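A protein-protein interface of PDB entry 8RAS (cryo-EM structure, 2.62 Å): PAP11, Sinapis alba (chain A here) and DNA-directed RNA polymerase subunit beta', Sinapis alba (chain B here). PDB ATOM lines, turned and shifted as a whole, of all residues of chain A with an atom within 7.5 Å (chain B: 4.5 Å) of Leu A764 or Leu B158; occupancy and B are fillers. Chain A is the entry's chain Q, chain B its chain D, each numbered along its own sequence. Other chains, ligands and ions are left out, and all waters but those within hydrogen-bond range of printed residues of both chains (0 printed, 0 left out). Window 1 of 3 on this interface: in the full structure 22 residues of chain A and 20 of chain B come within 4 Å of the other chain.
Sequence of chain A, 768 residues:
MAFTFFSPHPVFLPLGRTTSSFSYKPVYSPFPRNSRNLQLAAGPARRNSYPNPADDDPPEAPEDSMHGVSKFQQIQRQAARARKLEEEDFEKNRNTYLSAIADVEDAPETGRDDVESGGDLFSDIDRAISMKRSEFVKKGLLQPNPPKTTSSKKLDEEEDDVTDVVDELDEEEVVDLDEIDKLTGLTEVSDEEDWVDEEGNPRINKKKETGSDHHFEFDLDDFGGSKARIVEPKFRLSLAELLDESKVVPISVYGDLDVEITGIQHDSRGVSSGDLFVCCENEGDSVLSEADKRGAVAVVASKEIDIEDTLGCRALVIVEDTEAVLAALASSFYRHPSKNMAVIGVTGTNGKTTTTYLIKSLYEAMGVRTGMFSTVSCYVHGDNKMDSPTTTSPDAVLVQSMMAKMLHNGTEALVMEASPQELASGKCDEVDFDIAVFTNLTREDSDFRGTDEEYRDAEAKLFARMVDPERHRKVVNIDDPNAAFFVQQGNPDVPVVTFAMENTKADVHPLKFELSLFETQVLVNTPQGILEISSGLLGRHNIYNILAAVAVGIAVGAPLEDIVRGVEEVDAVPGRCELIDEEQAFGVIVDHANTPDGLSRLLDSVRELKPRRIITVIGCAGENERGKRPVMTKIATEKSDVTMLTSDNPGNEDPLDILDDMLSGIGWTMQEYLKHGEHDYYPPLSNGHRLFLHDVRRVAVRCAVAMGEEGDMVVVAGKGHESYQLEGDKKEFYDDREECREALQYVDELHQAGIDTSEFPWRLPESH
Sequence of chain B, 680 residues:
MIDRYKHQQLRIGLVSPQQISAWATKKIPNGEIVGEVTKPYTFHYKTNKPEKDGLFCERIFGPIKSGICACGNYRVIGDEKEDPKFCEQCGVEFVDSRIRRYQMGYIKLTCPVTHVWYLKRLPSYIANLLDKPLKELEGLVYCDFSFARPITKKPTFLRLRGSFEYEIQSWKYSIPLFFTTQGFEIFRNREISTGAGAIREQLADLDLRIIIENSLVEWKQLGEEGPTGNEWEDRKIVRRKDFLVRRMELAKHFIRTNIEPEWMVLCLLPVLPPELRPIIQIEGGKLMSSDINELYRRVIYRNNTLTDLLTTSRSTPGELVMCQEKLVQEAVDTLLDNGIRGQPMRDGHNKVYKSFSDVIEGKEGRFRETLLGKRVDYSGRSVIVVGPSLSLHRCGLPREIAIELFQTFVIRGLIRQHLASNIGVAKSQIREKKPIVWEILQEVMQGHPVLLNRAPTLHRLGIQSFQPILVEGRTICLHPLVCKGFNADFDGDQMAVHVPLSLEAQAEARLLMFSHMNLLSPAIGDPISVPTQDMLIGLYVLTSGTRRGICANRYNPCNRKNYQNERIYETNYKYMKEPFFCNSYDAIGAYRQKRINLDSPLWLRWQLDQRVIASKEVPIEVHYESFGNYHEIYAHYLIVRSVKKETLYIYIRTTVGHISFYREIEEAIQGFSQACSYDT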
ATOM      1  N   GLY A 677      15.147  -8.074  -9.591  1.00  0.00           N
ATOM      2  CA  GLY A 677      16.346  -8.691 -10.136  1.00  0.00           C
ATOM      3  C   GLY A 677      17.621  -7.999  -9.692  1.00  0.00           C
ATOM      4  O   GLY A 677      18.636  -8.653  -9.439  1.00  0.00           O
ATOM      5  N   ASP A 680      18.772  -9.093  -6.489  1.00  0.00           N
ATOM      6  CA  ASP A 680      18.994 -10.536  -6.571  1.00  0.00           C
ATOM      7  C   ASP A 680      18.129 -11.324  -5.593  1.00  0.00           C
ATOM      8  O   ASP A 680      18.580 -12.320  -5.018  1.00  0.00           O
ATOM      9  CB  ASP A 680      20.480 -10.873  -6.370  1.00  0.00           C
ATOM     10  CG  ASP A 680      21.039 -10.350  -5.058  1.00  0.00           C
ATOM     11  OD1 ASP A 680      20.646 -10.857  -3.987  1.00  0.00           O
ATOM     12  OD2 ASP A 680      21.880  -9.428  -5.100  1.00  0.00           O
ATOM     13  N   HIS A 694      11.952 -13.890 -18.336  1.00  0.00           N
ATOM     14  CA  HIS A 694      13.037 -13.581 -19.258  1.00  0.00           C
ATOM     15  C   HIS A 694      12.445 -13.194 -20.606  1.00  0.00           C
ATOM     16  O   HIS A 694      11.456 -13.782 -21.046  1.00  0.00           O
ATOM     17  CB  HIS A 694      13.998 -14.763 -19.414  1.00  0.00           C
ATOM     18  CG  HIS A 694      15.441 -14.365 -19.432  1.00  0.00           C
ATOM     19  ND1 HIS A 694      15.973 -13.540 -20.400  1.00  0.00           N
ATOM     20  CD2 HIS A 694      16.462 -14.671 -18.597  1.00  0.00           C
ATOM     21  CE1 HIS A 694      17.259 -13.359 -20.164  1.00  0.00           C
ATOM     22  NE2 HIS A 694      17.581 -14.035 -19.075  1.00  0.00           N
ATOM     23  N   LEU A 750      25.695 -28.344 -16.253  1.00  0.00           N
ATOM     24  CA  LEU A 750      25.394 -27.059 -15.633  1.00  0.00           C
ATOM     25  C   LEU A 750      25.171 -27.213 -14.135  1.00  0.00           C
ATOM     26  O   LEU A 750      25.629 -26.383 -13.342  1.00  0.00           O
ATOM     27  CB  LEU A 750      24.169 -26.435 -16.303  1.00  0.00           C
ATOM     28  CG  LEU A 750      23.734 -25.052 -15.824  1.00  0.00           C
ATOM     29  CD1 LEU A 750      24.846 -24.037 -16.032  1.00  0.00           C
ATOM     30  CD2 LEU A 750      22.468 -24.623 -16.544  1.00  0.00           C
ATOM     31  N   ALA A 753      28.565 -28.462 -12.124  1.00  0.00           N
ATOM     32  CA  ALA A 753      29.723 -27.581 -12.170  1.00  0.00           C
ATOM     33  C   ALA A 753      29.760 -26.589 -11.012  1.00  0.00           C
ATOM     34  O   ALA A 753      30.410 -25.543 -11.125  1.00  0.00           O
ATOM     35  CB  ALA A 753      29.765 -26.830 -13.502  1.00  0.00           C
ATOM     36  N   GLY A 754      29.082 -26.890  -9.907  1.00  0.00           N
ATOM     37  CA  GLY A 754      29.067 -26.009  -8.761  1.00  0.00           C
ATOM     38  C   GLY A 754      28.081 -24.865  -8.840  1.00  0.00           C
ATOM     39  O   GLY A 754      28.057 -24.028  -7.929  1.00  0.00           O
ATOM     40  N   ILE A 755      27.271 -24.799  -9.890  1.00  0.00           N
ATOM     41  CA  ILE A 755      26.296 -23.727 -10.059  1.00  0.00           C
ATOM     42  C   ILE A 755      24.958 -24.197  -9.507  1.00  0.00           C
ATOM     43  O   ILE A 755      24.408 -25.206  -9.961  1.00  0.00           O
ATOM     44  CB  ILE A 755      26.169 -23.318 -11.534  1.00  0.00           C
ATOM     45  CG1 ILE A 755      27.551 -23.187 -12.175  1.00  0.00           C
ATOM     46  CG2 ILE A 755      25.388 -22.019 -11.660  1.00  0.00           C
ATOM     47  CD1 ILE A 755      27.507 -22.887 -13.658  1.00  0.00           C
ATOM     48  N   ASP A 756      24.431 -23.465  -8.528  1.00  0.00           N
ATOM     49  CA  ASP A 756      23.115 -23.754  -7.965  1.00  0.00           C
ATOM     50  C   ASP A 756      22.074 -23.078  -8.846  1.00  0.00           C
ATOM     51  O   ASP A 756      21.607 -21.973  -8.567  1.00  0.00           O
ATOM     52  CB  ASP A 756      23.026 -23.278  -6.520  1.00  0.00           C
ATOM     53  CG  ASP A 756      21.677 -23.569  -5.890  1.00  0.00           C
ATOM     54  OD1 ASP A 756      20.979 -24.486  -6.372  1.00  0.00           O
ATOM     55  OD2 ASP A 756      21.317 -22.882  -4.913  1.00  0.00           O
ATOM     56  N   THR A 757      21.703 -23.755  -9.930  1.00  0.00           N
ATOM     57  CA  THR A 757      20.746 -23.229 -10.894  1.00  0.00           C
ATOM     58  C   THR A 757      19.302 -23.354 -10.425  1.00  0.00           C
ATOM     59  O   THR A 757      18.389 -23.160 -11.234  1.00  0.00           O
ATOM     60  CB  THR A 757      20.911 -23.940 -12.241  1.00  0.00           C
ATOM     61  OG1 THR A 757      20.095 -25.116 -12.267  1.00  0.00           O
ATOM     62  CG2 THR A 757      22.362 -24.338 -12.461  1.00  0.00           C
ATOM     63  N   GLU A 759      17.322 -21.538  -8.791  1.00  0.00           N
ATOM     64  CA  GLU A 759      16.480 -20.356  -8.896  1.00  0.00           C
ATOM     65  C   GLU A 759      17.321 -19.185  -9.379  1.00  0.00           C
ATOM     66  O   GLU A 759      18.553 -19.220  -9.335  1.00  0.00           O
ATOM     67  CB  GLU A 759      15.813 -20.017  -7.556  1.00  0.00           C
ATOM     68  CG  GLU A 759      16.750 -19.380  -6.542  1.00  0.00           C
ATOM     69  CD  GLU A 759      17.772 -20.355  -5.999  1.00  0.00           C
ATOM     70  OE1 GLU A 759      17.391 -21.501  -5.684  1.00  0.00           O
ATOM     71  OE2 GLU A 759      18.957 -19.978  -5.889  1.00  0.00           O
ATOM     72  N   PHE A 760      16.635 -18.153  -9.850  1.00  0.00           N
ATOM     73  CA  PHE A 760      17.293 -16.914 -10.246  1.00  0.00           C
ATOM     74  C   PHE A 760      17.517 -16.040  -9.017  1.00  0.00           C
ATOM     75  O   PHE A 760      16.569 -15.785  -8.267  1.00  0.00           O
ATOM     76  CB  PHE A 760      16.450 -16.158 -11.272  1.00  0.00           C
ATOM     77  CG  PHE A 760      16.395 -16.813 -12.626  1.00  0.00           C
ATOM     78  CD1 PHE A 760      17.129 -17.956 -12.897  1.00  0.00           C
ATOM     79  CD2 PHE A 760      15.599 -16.284 -13.628  1.00  0.00           C
ATOM     80  CE1 PHE A 760      17.072 -18.554 -14.142  1.00  0.00           C
ATOM     81  CE2 PHE A 760      15.538 -16.877 -14.875  1.00  0.00           C
ATOM     82  CZ  PHE A 760      16.275 -18.014 -15.131  1.00  0.00           C
ATOM     83  N   PRO A 761      18.745 -15.564  -8.774  1.00  0.00           N
ATOM     84  CA  PRO A 761      19.975 -15.780  -9.543  1.00  0.00           C
ATOM     85  C   PRO A 761      20.676 -17.086  -9.183  1.00  0.00           C
ATOM     86  O   PRO A 761      20.537 -17.582  -8.069  1.00  0.00           O
ATOM     87  CB  PRO A 761      20.816 -14.560  -9.164  1.00  0.00           C
ATOM     88  CG  PRO A 761      20.446 -14.308  -7.728  1.00  0.00           C
ATOM     89  CD  PRO A 761      18.990 -14.712  -7.595  1.00  0.00           C
ATOM     90  N   TRP A 762      21.438 -17.663 -10.108  1.00  0.00           N
ATOM     91  CA  TRP A 762      22.184 -18.879  -9.807  1.00  0.00           C
ATOM     92  C   TRP A 762      23.322 -18.567  -8.844  1.00  0.00           C
ATOM     93  O   TRP A 762      24.076 -17.610  -9.046  1.00  0.00           O
ATOM     94  CB  TRP A 762      22.732 -19.502 -11.090  1.00  0.00           C
ATOM     95  CG  TRP A 762      21.681 -19.868 -12.092  1.00  0.00           C
ATOM     96  CD1 TRP A 762      20.329 -19.833 -11.916  1.00  0.00           C
ATOM     97  CD2 TRP A 762      21.899 -20.324 -13.431  1.00  0.00           C
ATOM     98  NE1 TRP A 762      19.692 -20.238 -13.062  1.00  0.00           N
ATOM     99  CE2 TRP A 762      20.634 -20.544 -14.009  1.00  0.00           C
ATOM    100  CE3 TRP A 762      23.042 -20.566 -14.199  1.00  0.00           C
ATOM    101  CZ2 TRP A 762      20.479 -20.998 -15.315  1.00  0.00           C
ATOM    102  CZ3 TRP A 762      22.886 -21.015 -15.497  1.00  0.00           C
ATOM    103  CH2 TRP A 762      21.614 -21.224 -16.042  1.00  0.00           C
ATOM    104  N   ARG A 763      23.449 -19.379  -7.799  1.00  0.00           N
ATOM    105  CA  ARG A 763      24.483 -19.184  -6.784  1.00  0.00           C
ATOM    106  C   ARG A 763      25.799 -19.727  -7.326  1.00  0.00           C
ATOM    107  O   ARG A 763      26.144 -20.893  -7.139  1.00  0.00           O
ATOM    108  CB  ARG A 763      24.090 -19.864  -5.478  1.00  0.00           C
ATOM    109  CG  ARG A 763      24.414 -19.055  -4.231  1.00  0.00           C
ATOM    110  CD  ARG A 763      23.692 -17.713  -4.223  1.00  0.00           C
ATOM    111  NE  ARG A 763      22.328 -17.803  -4.731  1.00  0.00           N
ATOM    112  CZ  ARG A 763      21.311 -18.340  -4.069  1.00  0.00           C
ATOM    113  NH1 ARG A 763      21.463 -18.844  -2.856  1.00  0.00           N
ATOM    114  NH2 ARG A 763      20.109 -18.369  -4.640  1.00  0.00           N
ATOM    115  N   LEU A 764      26.541 -18.862  -8.014  1.00  0.00           N
ATOM    116  CA  LEU A 764      27.819 -19.257  -8.583  1.00  0.00           C
ATOM    117  C   LEU A 764      28.826 -19.540  -7.468  1.00  0.00           C
ATOM    118  O   LEU A 764      28.740 -18.960  -6.383  1.00  0.00           O
ATOM    119  CB  LEU A 764      28.352 -18.165  -9.508  1.00  0.00           C
ATOM    120  CG  LEU A 764      27.999 -18.233 -11.000  1.00  0.00           C
ATOM    121  CD1 LEU A 764      28.871 -19.246 -11.721  1.00  0.00           C
ATOM    122  CD2 LEU A 764      26.523 -18.540 -11.219  1.00  0.00           C
ATOM    123  N   PRO A 765      29.787 -20.439  -7.710  1.00  0.00           N
ATOM    124  CA  PRO A 765      30.741 -20.783  -6.638  1.00  0.00           C
ATOM    125  C   PRO A 765      31.548 -19.596  -6.138  1.00  0.00           C
ATOM    126  O   PRO A 765      31.633 -19.373  -4.923  1.00  0.00           O
ATOM    127  CB  PRO A 765      31.633 -21.847  -7.296  1.00  0.00           C
ATOM    128  CG  PRO A 765      30.829 -22.383  -8.430  1.00  0.00           C
ATOM    129  CD  PRO A 765      30.004 -21.240  -8.926  1.00  0.00           C
ATOM    130  N   GLU A 766      32.146 -18.826  -7.041  1.00  0.00           N
ATOM    131  CA  GLU A 766      33.007 -17.712  -6.673  1.00  0.00           C
ATOM    132  C   GLU A 766      32.261 -16.387  -6.573  1.00  0.00           C
ATOM    133  O   GLU A 766      32.893 -15.351  -6.348  1.00  0.00           O
ATOM    134  CB  GLU A 766      34.161 -17.589  -7.672  1.00  0.00           C
ATOM    135  CG  GLU A 766      33.730 -17.276  -9.094  1.00  0.00           C
ATOM    136  CD  GLU A 766      33.457 -18.523  -9.913  1.00  0.00           C
ATOM    137  OE1 GLU A 766      32.795 -19.447  -9.397  1.00  0.00           O
ATOM    138  OE2 GLU A 766      33.914 -18.583 -11.073  1.00  0.00           O
ATOM    139  N   SER A 767      30.940 -16.395  -6.738  1.00  0.00           N
ATOM    140  CA  SER A 767      30.119 -15.194  -6.623  1.00  0.00           C
ATOM    141  C   SER A 767      29.332 -15.276  -5.321  1.00  0.00           C
ATOM    142  O   SER A 767      28.430 -16.109  -5.186  1.00  0.00           O
ATOM    143  CB  SER A 767      29.184 -15.053  -7.821  1.00  0.00           C
ATOM    144  OG  SER A 767      27.918 -15.628  -7.548  1.00  0.00           O
ATOM    145  N   HIS A 768      29.674 -14.414  -4.369  1.00  0.00           N
ATOM    146  CA  HIS A 768      28.999 -14.390  -3.077  1.00  0.00           C
ATOM    147  C   HIS A 768      28.798 -12.958  -2.591  1.00  0.00           C
ATOM    148  O   HIS A 768      29.321 -12.013  -3.182  1.00  0.00           O
ATOM    149  CB  HIS A 768      29.793 -15.190  -2.041  1.00  0.00           C
ATOM    150  CG  HIS A 768      29.524 -16.662  -2.082  1.00  0.00           C
ATOM    151  ND1 HIS A 768      28.505 -17.248  -1.358  1.00  0.00           N
ATOM    152  CD2 HIS A 768      30.144 -17.660  -2.758  1.00  0.00           C
ATOM    153  CE1 HIS A 768      28.467 -18.555  -1.557  1.00  0.00           C
ATOM    154  N   ARG B 149      27.257  -7.688 -14.541  1.00  0.00           N
ATOM    155  CA  ARG B 149      26.009  -6.931 -14.543  1.00  0.00           C
ATOM    156  C   ARG B 149      26.240  -5.509 -15.041  1.00  0.00           C
ATOM    157  O   ARG B 149      26.179  -4.556 -14.255  1.00  0.00           O
ATOM    158  CB  ARG B 149      25.381  -6.911 -13.148  1.00  0.00           C
ATOM    159  CG  ARG B 149      23.898  -6.578 -13.142  1.00  0.00           C
ATOM    160  CD  ARG B 149      23.321  -6.663 -11.740  1.00  0.00           C
ATOM    161  NE  ARG B 149      23.915  -7.751 -10.972  1.00  0.00           N
ATOM    162  CZ  ARG B 149      23.242  -8.793 -10.508  1.00  0.00           C
ATOM    163  NH1 ARG B 149      21.942  -8.925 -10.717  1.00  0.00           N
ATOM    164  NH2 ARG B 149      23.888  -9.727  -9.816  1.00  0.00           N
ATOM    165  N   THR B 156      18.195 -10.357 -16.090  1.00  0.00           N
ATOM    166  CA  THR B 156      19.335 -11.259 -15.978  1.00  0.00           C
ATOM    167  C   THR B 156      18.951 -12.428 -15.079  1.00  0.00           C
ATOM    168  O   THR B 156      17.862 -12.462 -14.498  1.00  0.00           O
ATOM    169  CB  THR B 156      20.573 -10.539 -15.425  1.00  0.00           C
ATOM    170  OG1 THR B 156      20.368 -10.225 -14.042  1.00  0.00           O
ATOM    171  CG2 THR B 156      20.845  -9.258 -16.198  1.00  0.00           C
ATOM    172  N   PHE B 157      19.859 -13.405 -14.963  1.00  0.00           N
ATOM    173  CA  PHE B 157      19.587 -14.578 -14.139  1.00  0.00           C
ATOM    174  C   PHE B 157      20.804 -15.045 -13.346  1.00  0.00           C
ATOM    175  O   PHE B 157      20.841 -16.204 -12.916  1.00  0.00           O
ATOM    176  CB  PHE B 157      19.068 -15.735 -15.004  1.00  0.00           C
ATOM    177  CG  PHE B 157      19.993 -16.120 -16.125  1.00  0.00           C
ATOM    178  CD1 PHE B 157      21.068 -16.966 -15.901  1.00  0.00           C
ATOM    179  CD2 PHE B 157      19.789 -15.634 -17.403  1.00  0.00           C
ATOM    180  CE1 PHE B 157      21.919 -17.318 -16.928  1.00  0.00           C
ATOM    181  CE2 PHE B 157      20.638 -15.982 -18.435  1.00  0.00           C
ATOM    182  CZ  PHE B 157      21.702 -16.826 -18.197  1.00  0.00           C
ATOM    183  N   LEU B 158      21.797 -14.185 -13.131  1.00  0.00           N
ATOM    184  CA  LEU B 158      23.051 -14.591 -12.514  1.00  0.00           C
ATOM    185  C   LEU B 158      23.356 -13.712 -11.309  1.00  0.00           C
ATOM    186  O   LEU B 158      22.898 -12.571 -11.211  1.00  0.00           O
ATOM    187  CB  LEU B 158      24.209 -14.530 -13.517  1.00  0.00           C
ATOM    188  CG  LEU B 158      24.172 -15.590 -14.619  1.00  0.00           C
ATOM    189  CD1 LEU B 158      24.907 -15.111 -15.859  1.00  0.00           C
ATOM    190  CD2 LEU B 158      24.767 -16.897 -14.117  1.00  0.00           C
ATOM    191  N   ARG B 159      24.143 -14.264 -10.387  1.00  0.00           N
ATOM    192  CA  ARG B 159      24.552 -13.580  -9.162  1.00  0.00           C
ATOM    193  C   ARG B 159      25.955 -12.996  -9.308  1.00  0.00           C
ATOM    194  O   ARG B 159      26.756 -12.974  -8.369  1.00  0.00           O
ATOM    195  CB  ARG B 159      24.460 -14.539  -7.973  1.00  0.00           C
ATOM    196  CG  ARG B 159      24.710 -13.936  -6.587  1.00  0.00           C
ATOM    197  CD  ARG B 159      23.607 -14.284  -5.603  1.00  0.00           C
ATOM    198  NE  ARG B 159      23.451 -13.259  -4.576  1.00  0.00           N
ATOM    199  CZ  ARG B 159      23.788 -13.419  -3.304  1.00  0.00           C
ATOM    200  NH1 ARG B 159      24.313 -14.550  -2.864  1.00  0.00           N
ATOM    201  NH2 ARG B 159      23.594 -12.416  -2.451  1.00  0.00           N
ATOM    202  N   LEU B 160      26.286 -12.524 -10.504  1.00  0.00           N
ATOM    203  CA  LEU B 160      27.589 -11.929 -10.767  1.00  0.00           C
ATOM    204  C   LEU B 160      27.517 -10.429 -10.512  1.00  0.00           C
ATOM    205  O   LEU B 160      26.781  -9.712 -11.200  1.00  0.00           O
ATOM    206  CB  LEU B 160      28.030 -12.216 -12.200  1.00  0.00           C
ATOM    207  CG  LEU B 160      28.295 -13.685 -12.528  1.00  0.00           C
ATOM    208  CD1 LEU B 160      27.831 -14.006 -13.936  1.00  0.00           C
ATOM    209  CD2 LEU B 160      29.769 -14.012 -12.354  1.00  0.00           C
ATOM    210  N   SER B 170      33.441 -21.296 -14.908  1.00  0.00           N
ATOM    211  CA  SER B 170      32.204 -21.812 -15.482  1.00  0.00           C
ATOM    212  C   SER B 170      31.815 -21.040 -16.734  1.00  0.00           C
ATOM    213  O   SER B 170      31.369 -21.631 -17.724  1.00  0.00           O
ATOM    214  CB  SER B 170      31.081 -21.757 -14.446  1.00  0.00           C
ATOM    215  OG  SER B 170      30.682 -20.420 -14.203  1.00  0.00           O
ATOM    216  N   TRP B 171      31.986 -19.716 -16.715  1.00  0.00           N
ATOM    217  CA  TRP B 171      31.598 -18.891 -17.854  1.00  0.00           C
ATOM    218  C   TRP B 171      32.426 -19.184 -19.098  1.00  0.00           C
ATOM    219  O   TRP B 171      31.998 -18.843 -20.204  1.00  0.00           O
ATOM    220  CB  TRP B 171      31.719 -17.410 -17.491  1.00  0.00           C
ATOM    221  CG  TRP B 171      31.012 -16.491 -18.438  1.00  0.00           C
ATOM    222  CD1 TRP B 171      31.586 -15.617 -19.315  1.00  0.00           C
ATOM    223  CD2 TRP B 171      29.595 -16.337 -18.589  1.00  0.00           C
ATOM    224  NE1 TRP B 171      30.615 -14.938 -20.010  1.00  0.00           N
ATOM    225  CE2 TRP B 171      29.384 -15.361 -19.582  1.00  0.00           C
ATOM    226  CE3 TRP B 171      28.485 -16.933 -17.983  1.00  0.00           C
ATOM    227  CZ2 TRP B 171      28.110 -14.967 -19.983  1.00  0.00           C
ATOM    228  CZ3 TRP B 171      27.220 -16.541 -18.382  1.00  0.00           C
ATOM    229  CH2 TRP B 171      27.044 -15.568 -19.373  1.00  0.00           C
ATOM    230  N   GLU B 191      25.098  -9.640 -19.032  1.00  0.00           N
ATOM    231  CA  GLU B 191      25.446 -10.003 -17.663  1.00  0.00           C
ATOM    232  C   GLU B 191      26.937  -9.810 -17.429  1.00  0.00           C
ATOM    233  O   GLU B 191      27.356  -9.442 -16.328  1.00  0.00           O
ATOM    234  CB  GLU B 191      25.051 -11.453 -17.333  1.00  0.00           C
ATOM    235  CG  GLU B 191      23.695 -11.969 -17.856  1.00  0.00           C
ATOM    236  CD  GLU B 191      23.568 -11.986 -19.370  1.00  0.00           C
ATOM    237  OE1 GLU B 191      24.602 -11.850 -20.057  1.00  0.00           O
ATOM    238  OE2 GLU B 191      22.433 -12.130 -19.871  1.00  0.00           O
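The side-chain carboxylate (OD1) of Asp A680 lies within salt-bridge range of the guanidinium group (NH2) of Arg B159 (3.7 Å). O of Phe B157 is in hydrogen-bond range of N of Trp A762, at 3.2 Å. The side-chain hydroxyl of Ser A767 lies within hydrogen-bond range of the backbone carbonyl oxygen of Arg B159, at 3.0 Å.
N of Arg B149 lies within hydrogen-bond range of O of Glu B191 (2.5 Å). NH2 of Arg B149 sits at hydrogen-bond distance from O of Leu B160. The backbone carbonyl oxygen (O) of Leu B158 sits at hydrogen-bond distance from the guanidinium group (NH2) of Arg B149 (3.3 Å). O of Asp A756 lies within hydrogen-bond range of N of Arg A763.
O of Gly A677 touches NH1 of Arg B149, 3.6 Å away. Ser B170 touches Ile A755. Phe B157 touches Phe A760. Pro A761 touches Phe B157 (CA to O, 3.5 Å). Pro A761 touches Leu B158 (CB to C, 3.4 Å). Pro A761 touches Arg B159 (CB to N, 3.6 Å). Trp A762 touches Arg B159 (O to CB, 3.3 Å). Arg A763 touches Arg B159. CD2 of Leu B158 touches CD2 of Leu A764, 3.8 Å away. Leu A764 touches Ser B170.
Of the printed residues of chain B, Leu A764 touches Leu B158 (3.8 Å) and Ser B170 (3.3 Å). Of the printed residues of chain B, Pro A761 touches Phe B157, Leu B158 and Arg B159. Of the printed residues of chain B, Ser A767 touches Arg B159. The nearest printed residue of chain B that does not touch Leu A764 is Leu B160 (4.8 Å).
Hydrophobic or aromatic side chains of chain B within 4 Å of the printed part of chain A: Phe B157 and Leu B158. Along chain B the printed residues that touch a printed residue of chain A span positions 149 to 170. Of the 19 printed residues of chain A, 10 touch a printed residue of chain B. Hydrophobic or aromatic side chains of chain A that line the printed part of chain B: His A694, Ile A755, Phe A760, Pro A761, Trp A762 and Leu A764. Among the printed residues, Asp or Glu carboxylates within 4 Å of a Lys or Arg side-chain nitrogen of the other chain: Asp A680 with Arg B159.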
